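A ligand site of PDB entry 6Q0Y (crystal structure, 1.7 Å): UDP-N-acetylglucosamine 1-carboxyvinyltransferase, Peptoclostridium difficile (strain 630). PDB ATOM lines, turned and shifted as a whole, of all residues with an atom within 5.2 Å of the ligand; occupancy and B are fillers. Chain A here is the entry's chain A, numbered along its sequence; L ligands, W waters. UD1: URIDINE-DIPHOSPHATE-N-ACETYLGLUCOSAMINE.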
ATOM      1  N   LYS A  26      20.744 -13.981   0.822  1.00  0.00           N
ATOM      2  CA  LYS A  26      20.262 -14.791   1.944  1.00  0.00           C
ATOM      3  C   LYS A  26      18.846 -14.345   2.314  1.00  0.00           C
ATOM      4  O   LYS A  26      17.951 -15.196   2.470  1.00  0.00           O
ATOM      5  CB  LYS A  26      21.187 -14.738   3.167  1.00  0.00           C
ATOM      6  CG  LYS A  26      20.651 -15.582   4.291  1.00  0.00           C
ATOM      7  CD  LYS A  26      21.569 -15.716   5.488  1.00  0.00           C
ATOM      8  CE  LYS A  26      21.593 -14.482   6.380  1.00  0.00           C
ATOM      9  NZ  LYS A  26      20.267 -14.156   6.949  1.00  0.00           N
ATOM     10  N   ASN A  27      18.627 -13.052   2.424  1.00  0.00           N
ATOM     11  CA  ASN A  27      17.338 -12.611   2.982  1.00  0.00           C
ATOM     12  C   ASN A  27      16.259 -12.588   1.897  1.00  0.00           C
ATOM     13  O   ASN A  27      15.091 -12.385   2.256  1.00  0.00           O
ATOM     14  CB  ASN A  27      17.564 -11.288   3.695  1.00  0.00           C
ATOM     15  CG  ASN A  27      18.339 -11.522   4.974  1.00  0.00           C
ATOM     16  OD1 ASN A  27      18.456 -12.643   5.435  1.00  0.00           O
ATOM     17  ND2 ASN A  27      18.866 -10.463   5.552  1.00  0.00           N
ATOM     18  N   LEU A  30      15.420 -16.937   1.799  1.00  0.00           N
ATOM     19  CA  LEU A  30      14.769 -17.611   2.921  1.00  0.00           C
ATOM     20  C   LEU A  30      13.249 -17.455   2.827  1.00  0.00           C
ATOM     21  O   LEU A  30      12.510 -18.435   2.848  1.00  0.00           O
ATOM     22  CB  LEU A  30      15.367 -17.129   4.255  1.00  0.00           C
ATOM     23  CG  LEU A  30      16.836 -17.483   4.490  1.00  0.00           C
ATOM     24  CD1 LEU A  30      17.364 -16.841   5.774  1.00  0.00           C
ATOM     25  CD2 LEU A  30      17.063 -18.984   4.564  1.00  0.00           C
ATOM     26  N   ARG A  96      15.925 -18.208  13.201  1.00  0.00           N
ATOM     27  CA  ARG A  96      14.570 -17.700  13.531  1.00  0.00           C
ATOM     28  C   ARG A  96      13.777 -17.440  12.235  1.00  0.00           C
ATOM     29  O   ARG A  96      12.540 -17.397  12.333  1.00  0.00           O
ATOM     30  CB  ARG A  96      14.599 -16.454  14.421  1.00  0.00           C
ATOM     31  CG  ARG A  96      15.307 -15.253  13.826  1.00  0.00           C
ATOM     32  CD  ARG A  96      15.277 -14.058  14.773  1.00  0.00           C
ATOM     33  NE  ARG A  96      13.980 -13.380  14.919  1.00  0.00           N
ATOM     34  CZ  ARG A  96      13.333 -13.216  16.071  1.00  0.00           C
ATOM     35  NH1 ARG A  96      13.867 -13.649  17.200  1.00  0.00           N
ATOM     36  NH2 ARG A  96      12.165 -12.602  16.087  1.00  0.00           N
ATOM     37  N   ALA A  97      14.427 -17.266  11.099  1.00  0.00           N
ATOM     38  CA  ALA A  97      13.713 -17.103   9.802  1.00  0.00           C
ATOM     39  C   ALA A  97      12.837 -18.333   9.498  1.00  0.00           C
ATOM     40  O   ALA A  97      11.932 -18.241   8.599  1.00  0.00           O
ATOM     41  CB  ALA A  97      14.692 -16.814   8.704  1.00  0.00           C
ATOM     42  N   LEU A 100       9.066 -17.975   9.099  1.00  0.00           N
ATOM     43  CA  LEU A 100       8.436 -17.590   7.796  1.00  0.00           C
ATOM     44  C   LEU A 100       7.645 -18.736   7.164  1.00  0.00           C
ATOM     45  O   LEU A 100       6.921 -18.472   6.184  1.00  0.00           O
ATOM     46  CB  LEU A 100       9.482 -17.045   6.835  1.00  0.00           C
ATOM     47  CG  LEU A 100      10.186 -15.795   7.342  1.00  0.00           C
ATOM     48  CD1 LEU A 100      11.362 -15.438   6.433  1.00  0.00           C
ATOM     49  CD2 LEU A 100       9.182 -14.644   7.502  1.00  0.00           C
ATOM     50  N   ILE A 122      20.884  -9.950  18.453  1.00  0.00           N
ATOM     51  CA  ILE A 122      20.881  -8.491  18.191  1.00  0.00           C
ATOM     52  C   ILE A 122      19.669  -7.805  18.808  1.00  0.00           C
ATOM     53  O   ILE A 122      19.474  -6.593  18.573  1.00  0.00           O
ATOM     54  CB  ILE A 122      20.964  -8.223  16.693  1.00  0.00           C
ATOM     55  CG1 ILE A 122      19.786  -8.837  15.941  1.00  0.00           C
ATOM     56  CG2 ILE A 122      22.300  -8.690  16.163  1.00  0.00           C
ATOM     57  CD1 ILE A 122      19.714  -8.378  14.508  1.00  0.00           C
ATOM     58  N   THR A 124      15.788  -8.245  21.447  1.00  0.00           N
ATOM     59  CA  THR A 124      14.450  -8.816  21.727  1.00  0.00           C
ATOM     60  C   THR A 124      13.599  -8.521  20.503  1.00  0.00           C
ATOM     61  O   THR A 124      13.441  -7.326  20.138  1.00  0.00           O
ATOM     62  CB  THR A 124      13.768  -8.148  22.928  1.00  0.00           C
ATOM     63  OG1 THR A 124      14.699  -8.202  24.017  1.00  0.00           O
ATOM     64  CG2 THR A 124      12.439  -8.797  23.285  1.00  0.00           C
ATOM     65  N   ARG A 125      13.156  -9.559  19.839  1.00  0.00           N
ATOM     66  CA  ARG A 125      12.487  -9.398  18.535  1.00  0.00           C
ATOM     67  C   ARG A 125      11.170 -10.159  18.597  1.00  0.00           C
ATOM     68  O   ARG A 125      11.138 -11.357  18.294  1.00  0.00           O
ATOM     69  CB  ARG A 125      13.455  -9.901  17.471  1.00  0.00           C
ATOM     70  CG  ARG A 125      14.697  -9.021  17.301  1.00  0.00           C
ATOM     71  CD  ARG A 125      15.800  -9.709  16.532  1.00  0.00           C
ATOM     72  NE  ARG A 125      15.394  -9.998  15.165  1.00  0.00           N
ATOM     73  CZ  ARG A 125      16.123 -10.695  14.302  1.00  0.00           C
ATOM     74  NH1 ARG A 125      15.707 -10.868  13.069  1.00  0.00           N
ATOM     75  NH2 ARG A 125      17.307 -11.159  14.664  1.00  0.00           N
ATOM     76  N   PRO A 126      10.076  -9.467  18.965  1.00  0.00           N
ATOM     77  CA  PRO A 126       8.766 -10.106  19.036  1.00  0.00           C
ATOM     78  C   PRO A 126       8.251 -10.417  17.636  1.00  0.00           C
ATOM     79  O   PRO A 126       8.764  -9.858  16.682  1.00  0.00           O
ATOM     80  CB  PRO A 126       7.837  -9.096  19.704  1.00  0.00           C
ATOM     81  CG  PRO A 126       8.627  -7.802  19.842  1.00  0.00           C
ATOM     82  CD  PRO A 126      10.038  -8.056  19.363  1.00  0.00           C
ATOM     83  N   ILE A 127       7.259 -11.301  17.553  1.00  0.00           N
ATOM     84  CA  ILE A 127       6.603 -11.603  16.248  1.00  0.00           C
ATOM     85  C   ILE A 127       5.116 -11.241  16.351  1.00  0.00           C
ATOM     86  O   ILE A 127       4.314 -11.741  15.502  1.00  0.00           O
ATOM     87  CB  ILE A 127       6.862 -13.059  15.824  1.00  0.00           C
ATOM     88  CG1 ILE A 127       6.609 -14.066  16.940  1.00  0.00           C
ATOM     89  CG2 ILE A 127       8.264 -13.225  15.278  1.00  0.00           C
ATOM     90  CD1 ILE A 127       5.190 -14.183  17.386  1.00  0.00           C
ATOM     91  N   ASP A 128       4.779 -10.314  17.252  1.00  0.00           N
ATOM     92  CA  ASP A 128       3.381  -9.827  17.483  1.00  0.00           C
ATOM     93  C   ASP A 128       2.750  -9.354  16.162  1.00  0.00           C
ATOM     94  O   ASP A 128       1.533  -9.542  15.992  1.00  0.00           O
ATOM     95  CB  ASP A 128       3.319  -8.708  18.523  1.00  0.00           C
ATOM     96  CG  ASP A 128       4.112  -7.446  18.148  1.00  0.00           C
ATOM     97  OD1 ASP A 128       3.491  -6.364  18.073  1.00  0.00           O
ATOM     98  OD2 ASP A 128       5.345  -7.528  17.970  1.00  0.00           O
ATOM     99  N   LEU A 129       3.471  -8.702  15.273  1.00  0.00           N
ATOM    100  CA  LEU A 129       2.848  -8.136  14.050  1.00  0.00           C
ATOM    101  C   LEU A 129       2.497  -9.262  13.080  1.00  0.00           C
ATOM    102  O   LEU A 129       1.562  -9.115  12.285  1.00  0.00           O
ATOM    103  CB  LEU A 129       3.781  -7.128  13.385  1.00  0.00           C
ATOM    104  CG  LEU A 129       4.035  -5.868  14.210  1.00  0.00           C
ATOM    105  CD1 LEU A 129       5.063  -4.982  13.530  1.00  0.00           C
ATOM    106  CD2 LEU A 129       2.743  -5.106  14.433  1.00  0.00           C
ATOM    107  N   HIS A 130       3.253 -10.358  13.095  1.00  0.00           N
ATOM    108  CA  HIS A 130       2.907 -11.503  12.231  1.00  0.00           C
ATOM    109  C   HIS A 130       1.524 -12.005  12.651  1.00  0.00           C
ATOM    110  O   HIS A 130       0.616 -12.191  11.807  1.00  0.00           O
ATOM    111  CB  HIS A 130       3.942 -12.615  12.421  1.00  0.00           C
ATOM    112  CG  HIS A 130       5.317 -12.256  11.994  1.00  0.00           C
ATOM    113  ND1 HIS A 130       5.999 -12.992  11.088  1.00  0.00           N
ATOM    114  CD2 HIS A 130       6.172 -11.319  12.436  1.00  0.00           C
ATOM    115  CE1 HIS A 130       7.223 -12.514  10.944  1.00  0.00           C
ATOM    116  NE2 HIS A 130       7.366 -11.485  11.753  1.00  0.00           N
ATOM    117  N   PHE A 164       4.886  -1.230  12.718  1.00  0.00           N
ATOM    118  CA  PHE A 164       6.266  -0.985  12.233  1.00  0.00           C
ATOM    119  C   PHE A 164       6.360  -1.730  10.917  1.00  0.00           C
ATOM    120  O   PHE A 164       5.752  -2.788  10.830  1.00  0.00           O
ATOM    121  CB  PHE A 164       7.300  -1.489  13.244  1.00  0.00           C
ATOM    122  CG  PHE A 164       8.728  -1.136  12.883  1.00  0.00           C
ATOM    123  CD1 PHE A 164       9.276   0.080  13.258  1.00  0.00           C
ATOM    124  CD2 PHE A 164       9.498  -1.985  12.092  1.00  0.00           C
ATOM    125  CE1 PHE A 164      10.573   0.433  12.893  1.00  0.00           C
ATOM    126  CE2 PHE A 164      10.780  -1.615  11.709  1.00  0.00           C
ATOM    127  CZ  PHE A 164      11.344  -0.431  12.145  1.00  0.00           C
ATOM    128  N   PRO A 165       7.053  -1.187   9.896  1.00  0.00           N
ATOM    129  CA  PRO A 165       7.154  -1.820   8.579  1.00  0.00           C
ATOM    130  C   PRO A 165       8.099  -3.018   8.681  1.00  0.00           C
ATOM    131  O   PRO A 165       9.189  -3.039   8.080  1.00  0.00           O
ATOM    132  CB  PRO A 165       7.603  -0.661   7.678  1.00  0.00           C
ATOM    133  CG  PRO A 165       8.435   0.196   8.574  1.00  0.00           C
ATOM    134  CD  PRO A 165       7.694   0.121   9.886  1.00  0.00           C
ATOM    135  N   SER A 166       7.663  -4.018   9.447  1.00  0.00           N
ATOM    136  CA  SER A 166       8.418  -5.275   9.678  1.00  0.00           C
ATOM    137  C   SER A 166       8.599  -6.015   8.350  1.00  0.00           C
ATOM    138  O   SER A 166       7.617  -6.330   7.640  1.00  0.00           O
ATOM    139  CB  SER A 166       7.739  -6.140  10.718  1.00  0.00           C
ATOM    140  OG  SER A 166       8.206  -7.497  10.679  1.00  0.00           O
ATOM    141  N   VAL A 167       9.850  -6.351   8.045  1.00  0.00           N
ATOM    142  CA  VAL A 167      10.190  -7.189   6.878  1.00  0.00           C
ATOM    143  C   VAL A 167       9.486  -8.557   7.013  1.00  0.00           C
ATOM    144  O   VAL A 167       8.703  -8.967   6.107  1.00  0.00           O
ATOM    145  CB  VAL A 167      11.707  -7.342   6.770  1.00  0.00           C
ATOM    146  CG1 VAL A 167      12.108  -8.360   5.723  1.00  0.00           C
ATOM    147  CG2 VAL A 167      12.322  -5.987   6.466  1.00  0.00           C
ATOM    148  N   GLY A 168       9.767  -9.236   8.106  1.00  0.00           N
ATOM    149  CA  GLY A 168       9.215 -10.588   8.311  1.00  0.00           C
ATOM    150  C   GLY A 168       7.691 -10.596   8.338  1.00  0.00           C
ATOM    151  O   GLY A 168       7.083 -11.541   7.805  1.00  0.00           O
ATOM    152  N   ALA A 169       7.076  -9.637   8.999  1.00  0.00           N
ATOM    153  CA  ALA A 169       5.606  -9.641   9.134  1.00  0.00           C
ATOM    154  C   ALA A 169       4.998  -9.372   7.757  1.00  0.00           C
ATOM    155  O   ALA A 169       4.014 -10.021   7.384  1.00  0.00           O
ATOM    156  CB  ALA A 169       5.168  -8.601  10.118  1.00  0.00           C
ATOM    157  N   GLU A 171       6.318 -10.231   4.895  1.00  0.00           N
ATOM    158  CA  GLU A 171       6.489 -11.490   4.135  1.00  0.00           C
ATOM    159  C   GLU A 171       5.457 -12.510   4.570  1.00  0.00           C
ATOM    160  O   GLU A 171       4.800 -13.132   3.708  1.00  0.00           O
ATOM    161  CB  GLU A 171       7.891 -12.033   4.336  1.00  0.00           C
ATOM    162  CG  GLU A 171       8.944 -11.152   3.711  1.00  0.00           C
ATOM    163  CD  GLU A 171      10.386 -11.294   4.144  1.00  0.00           C
ATOM    164  OE1 GLU A 171      10.654 -11.867   5.213  1.00  0.00           O
ATOM    165  OE2 GLU A 171      11.241 -10.781   3.398  1.00  0.00           O
ATOM    166  N   GLU A 192      11.527  -3.070   1.623  1.00  0.00           N
ATOM    167  CA  GLU A 192      12.807  -3.763   1.302  1.00  0.00           C
ATOM    168  C   GLU A 192      12.726  -4.495  -0.025  1.00  0.00           C
ATOM    169  O   GLU A 192      11.707  -5.083  -0.389  1.00  0.00           O
ATOM    170  CB  GLU A 192      13.235  -4.759   2.375  1.00  0.00           C
ATOM    171  CG  GLU A 192      14.042  -4.150   3.503  1.00  0.00           C
ATOM    172  CD  GLU A 192      13.338  -3.210   4.466  1.00  0.00           C
ATOM    173  OE1 GLU A 192      12.084  -3.154   4.451  1.00  0.00           O
ATOM    174  OE2 GLU A 192      14.075  -2.513   5.238  1.00  0.00           O
ATOM    175  N   THR A 307      20.262  -1.520   8.705  1.00  0.00           N
ATOM    176  CA  THR A 307      20.834  -1.993   9.994  1.00  0.00           C
ATOM    177  C   THR A 307      21.842  -3.111   9.713  1.00  0.00           C
ATOM    178  O   THR A 307      22.796  -3.258  10.468  1.00  0.00           O
ATOM    179  CB  THR A 307      19.724  -2.373  10.987  1.00  0.00           C
ATOM    180  OG1 THR A 307      20.322  -2.892  12.174  1.00  0.00           O
ATOM    181  CG2 THR A 307      18.718  -3.367  10.457  1.00  0.00           C
ATOM    182  N   ASP A 308      21.654  -3.875   8.632  1.00  0.00           N
ATOM    183  CA  ASP A 308      22.565  -5.010   8.323  1.00  0.00           C
ATOM    184  C   ASP A 308      23.933  -4.496   7.823  1.00  0.00           C
ATOM    185  O   ASP A 308      24.826  -5.344   7.649  1.00  0.00           O
ATOM    186  CB  ASP A 308      21.981  -6.015   7.325  1.00  0.00           C
ATOM    187  CG  ASP A 308      20.900  -6.928   7.930  1.00  0.00           C
ATOM    188  OD1 ASP A 308      20.140  -7.525   7.159  1.00  0.00           O
ATOM    189  OD2 ASP A 308      20.841  -7.034   9.182  1.00  0.00           O
ATOM    190  N   VAL A 330      16.505   0.498  14.418  1.00  0.00           N
ATOM    191  CA  VAL A 330      15.725  -0.681  13.977  1.00  0.00           C
ATOM    192  C   VAL A 330      15.817  -1.785  15.024  1.00  0.00           C
ATOM    193  O   VAL A 330      14.770  -2.356  15.355  1.00  0.00           O
ATOM    194  CB  VAL A 330      16.138  -1.164  12.585  1.00  0.00           C
ATOM    195  CG1 VAL A 330      15.355  -2.421  12.162  1.00  0.00           C
ATOM    196  CG2 VAL A 330      15.961  -0.044  11.579  1.00  0.00           C
ATOM    197  N   PHE A 331      16.989  -2.041  15.589  1.00  0.00           N
ATOM    198  CA  PHE A 331      17.175  -3.093  16.607  1.00  0.00           C
ATOM    199  C   PHE A 331      17.529  -2.466  17.968  1.00  0.00           C
ATOM    200  O   PHE A 331      18.051  -1.395  17.978  1.00  0.00           O
ATOM    201  CB  PHE A 331      18.191  -4.113  16.111  1.00  0.00           C
ATOM    202  CG  PHE A 331      17.571  -5.057  15.121  1.00  0.00           C
ATOM    203  CD1 PHE A 331      16.574  -5.939  15.511  1.00  0.00           C
ATOM    204  CD2 PHE A 331      17.968  -5.040  13.792  1.00  0.00           C
ATOM    205  CE1 PHE A 331      16.005  -6.802  14.592  1.00  0.00           C
ATOM    206  CE2 PHE A 331      17.403  -5.903  12.883  1.00  0.00           C
ATOM    207  CZ  PHE A 331      16.441  -6.803  13.282  1.00  0.00           C
ATOM    208  N   GLU A 332      17.255  -3.134  19.097  1.00  0.00           N
ATOM    209  CA  GLU A 332      17.510  -2.480  20.418  1.00  0.00           C
ATOM    210  C   GLU A 332      18.981  -2.583  20.794  1.00  0.00           C
ATOM    211  O   GLU A 332      19.630  -1.543  21.048  1.00  0.00           O
ATOM    212  CB  GLU A 332      16.719  -3.097  21.577  1.00  0.00           C
ATOM    213  CG  GLU A 332      15.247  -3.296  21.289  1.00  0.00           C
ATOM    214  CD  GLU A 332      14.881  -4.756  21.111  1.00  0.00           C
ATOM    215  OE1 GLU A 332      15.665  -5.636  21.549  1.00  0.00           O
ATOM    216  OE2 GLU A 332      13.803  -5.003  20.529  1.00  0.00           O
ATOM    217  N   ARG A 334      21.931  -3.673  19.095  1.00  0.00           N
ATOM    218  CA  ARG A 334      22.814  -4.110  17.983  1.00  0.00           C
ATOM    219  C   ARG A 334      24.162  -3.373  18.115  1.00  0.00           C
ATOM    220  O   ARG A 334      24.714  -2.960  17.147  1.00  0.00           O
ATOM    221  CB  ARG A 334      22.122  -4.008  16.617  1.00  0.00           C
ATOM    222  CG  ARG A 334      22.840  -4.779  15.529  1.00  0.00           C
ATOM    223  CD  ARG A 334      22.059  -4.808  14.229  1.00  0.00           C
ATOM    224  NE  ARG A 334      22.618  -5.862  13.382  1.00  0.00           N
ATOM    225  CZ  ARG A 334      22.095  -6.265  12.261  1.00  0.00           C
ATOM    226  NH1 ARG A 334      21.035  -5.633  11.818  1.00  0.00           N
ATOM    227  NH2 ARG A 334      22.591  -7.330  11.621  1.00  0.00           N
HETATM  228  C1' UD1 L   1      14.982  -9.159   8.560  1.00  0.00           C
HETATM  229  C2' UD1 L   1      16.336  -9.751   8.193  1.00  0.00           C
HETATM  230  C3' UD1 L   1      17.426  -9.225   9.146  1.00  0.00           C
HETATM  231  C4' UD1 L   1      17.460  -7.708   9.037  1.00  0.00           C
HETATM  232  C5' UD1 L   1      16.047  -7.179   9.335  1.00  0.00           C
HETATM  233  C6' UD1 L   1      15.908  -5.640   9.257  1.00  0.00           C
HETATM  234  C7' UD1 L   1      15.752 -11.879   7.196  1.00  0.00           C
HETATM  235  C8' UD1 L   1      15.643 -13.353   7.458  1.00  0.00           C
HETATM  236  N2' UD1 L   1      16.274 -11.195   8.200  1.00  0.00           N
HETATM  237  O1' UD1 L   1      14.695  -9.479   9.903  1.00  0.00           O
HETATM  238  O3' UD1 L   1      18.687  -9.845   8.891  1.00  0.00           O
HETATM  239  O4' UD1 L   1      18.384  -7.223  10.024  1.00  0.00           O
HETATM  240  O5' UD1 L   1      15.063  -7.762   8.433  1.00  0.00           O
HETATM  241  O6' UD1 L   1      16.451  -5.154   8.009  1.00  0.00           O
HETATM  242  O7' UD1 L   1      15.367 -11.336   6.153  1.00  0.00           O
HETATM  243  N1  UD1 L   1       9.308  -6.265  15.161  1.00  0.00           N
HETATM  244  C2  UD1 L   1       8.297  -6.260  16.108  1.00  0.00           C
HETATM  245  N3  UD1 L   1       7.246  -7.124  15.874  1.00  0.00           N
HETATM  246  C4  UD1 L   1       7.194  -8.054  14.852  1.00  0.00           C
HETATM  247  C5  UD1 L   1       8.293  -8.045  13.934  1.00  0.00           C
HETATM  248  C6  UD1 L   1       9.303  -7.172  14.109  1.00  0.00           C
HETATM  249  O2  UD1 L   1       8.279  -5.463  17.039  1.00  0.00           O
HETATM  250  O4  UD1 L   1       6.234  -8.820  14.833  1.00  0.00           O
HETATM  251  C1B UD1 L   1      10.441  -5.341  15.349  1.00  0.00           C
HETATM  252  C2B UD1 L   1      11.728  -6.124  15.633  1.00  0.00           C
HETATM  253  O2' UD1 L   1      11.947  -6.427  16.998  1.00  0.00           O
HETATM  254  C3B UD1 L   1      12.781  -5.134  15.128  1.00  0.00           C
HETATM  255  C4B UD1 L   1      12.079  -4.381  14.006  1.00  0.00           C
HETATM  256  O4B UD1 L   1      10.655  -4.628  14.153  1.00  0.00           O
HETATM  257  O3B UD1 L   1      13.120  -4.213  16.151  1.00  0.00           O
HETATM  258  C5B UD1 L   1      12.502  -4.783  12.614  1.00  0.00           C
HETATM  259  O5B UD1 L   1      12.387  -6.216  12.479  1.00  0.00           O
HETATM  260  PA  UD1 L   1      11.941  -6.889  11.070  1.00  0.00           P
HETATM  261  O1A UD1 L   1      10.736  -7.753  11.376  1.00  0.00           O
HETATM  262  O2A UD1 L   1      11.864  -5.821  10.021  1.00  0.00           O
HETATM  263  O3A UD1 L   1      13.187  -7.843  10.836  1.00  0.00           O
HETATM  264  PB  UD1 L   1      13.204  -9.432  10.503  1.00  0.00           P
HETATM  265  O1B UD1 L   1      12.191  -9.718   9.406  1.00  0.00           O
HETATM  266  O2B UD1 L   1      13.229 -10.161  11.803  1.00  0.00           O
HETATM  267  O   HOH W   1      15.034  -2.826   7.762  1.00  0.00           O
HETATM  268  O   HOH W   2      16.279  -6.387   5.556  1.00  0.00           O
HETATM  269  O   HOH W   3      12.349 -12.041   7.995  1.00  0.00           O
HETATM  270  O   HOH W   4       9.908 -10.354  11.942  1.00  0.00           O
HETATM  271  O   HOH W   5      16.503 -13.104  10.853  1.00  0.00           O
HETATM  272  O   HOH W   6      12.810  -3.302   9.192  1.00  0.00           O
HETATM  273  O   HOH W   7      13.799 -10.787   4.097  1.00  0.00           O
HETATM  274  O   HOH W   8      19.066  -4.241   6.987  1.00  0.00           O
HETATM  275  O   HOH W   9      12.862  -9.033  14.200  1.00  0.00           O
HETATM  276  O   HOH W  10      11.179  -4.724  18.944  1.00  0.00           O
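OD2 of Asp 308 sits at hydrogen-bond distance from O4' of the ligand (2.6 Å). The backbone carbonyl oxygen (O) of Val 330 lies within hydrogen-bond range of an oxygen (O3B) of the ligand, at 2.6 Å. The side-chain hydroxyl of Ser 166 is in hydrogen-bond range of an oxygen (O1A) of the ligand (2.6 Å). The backbone NH (N) of Gly 168 is in hydrogen-bond range of an oxygen (O1B) of the ligand, 2.8 Å away. N of Leu 129 is in hydrogen-bond range of O4 of the ligand (2.8 Å). N of Asp 128 sits at hydrogen-bond distance from O4 of the ligand (3.2 Å). OD2 of Asp 128 is in hydrogen-bond range of N3 of the ligand (2.9 Å). O2B of the ligand is in salt-bridge range of NH1 of Arg 125. An oxygen (O2A) of the ligand lies within hydrogen-bond range of the backbone NH (N) of Val 167 (2.9 Å). A nitrogen (N3) of the ligand sits close to the backbone carbonyl oxygen of Pro 126. O3' of the ligand lies within hydrogen-bond range of ND2 of Asn 27, at 3.4 Å.
OD2 of Asp 308 is in salt-bridge range of NH1 of Arg 334. OG of Ser 166 sits close to N of Gly 168 (3.5 Å). OG of Ser 166 sits at hydrogen-bond distance from N of Ala 169, 2.9 Å away. NH2 of Arg 96 sits at hydrogen-bond distance from O of Arg 125 (2.7 Å). OD1 of Asn 27 lies within hydrogen-bond range of NZ of Lys 26 (2.8 Å). The backbone NH (N) of Ala 169 lies within hydrogen-bond range of a ring nitrogen (NE2) of His 130 (3.3 Å). The guanidinium group of Arg 334 is in hydrogen-bond range of the side-chain hydroxyl of Thr 307 (2.9 Å). The backbone NH (N) of Thr 124 lies within hydrogen-bond range of the side-chain carboxylate (OE1) of Glu 332 (2.6 Å).
Ala 97 touches the ligand. Thr 124 touches the ligand. Ile 127 touches the ligand (C to O4, 3.1 Å). His 130 touches the ligand. Phe 164 touches the ligand. CG2 of Thr 307 touches O6' of the ligand, at 3.8 Å. Phe 331 touches the ligand (CE2 to O4', 3.3 Å). NH1 of Arg 334 touches O4' of the ligand (3.6 Å). Within 4 Å of the ligand: Asn 27, Ala 97, Thr 124, Arg 125, Pro 126, Ile 127, Asp 128, Leu 129, His 130, Phe 164, Ser 166, Val 167, Gly 168, Thr 307, Asp 308, Val 330, Phe 331 and Arg 334. The nearest printed residue that does not touch the ligand is Glu 332 (4.2 Å).
Water W10 bridges O2' of the ligand (2.7 Å) and OE2 of Glu 332 (3.1 Å). Water W3 bridges O1B of the ligand (2.7 Å) and OE1 of Glu 171 (3.3 Å). Water W1 bridges OE2 of Glu 192 (2.7 Å) and O6' of the ligand (2.7 Å). Water W4 lies within hydrogen-bond range of O1A of the ligand (2.8 Å) and NE2 of His 130 (2.8 Å). Water W8 lies within hydrogen-bond range of an oxygen (O6') of the ligand, the backbone NH (N) of Asp 308 and the backbone NH (N) of Thr 307. Water W5 bridges NH1 of Arg 125 (3.2 Å) and N2' of the ligand (3.3 Å).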
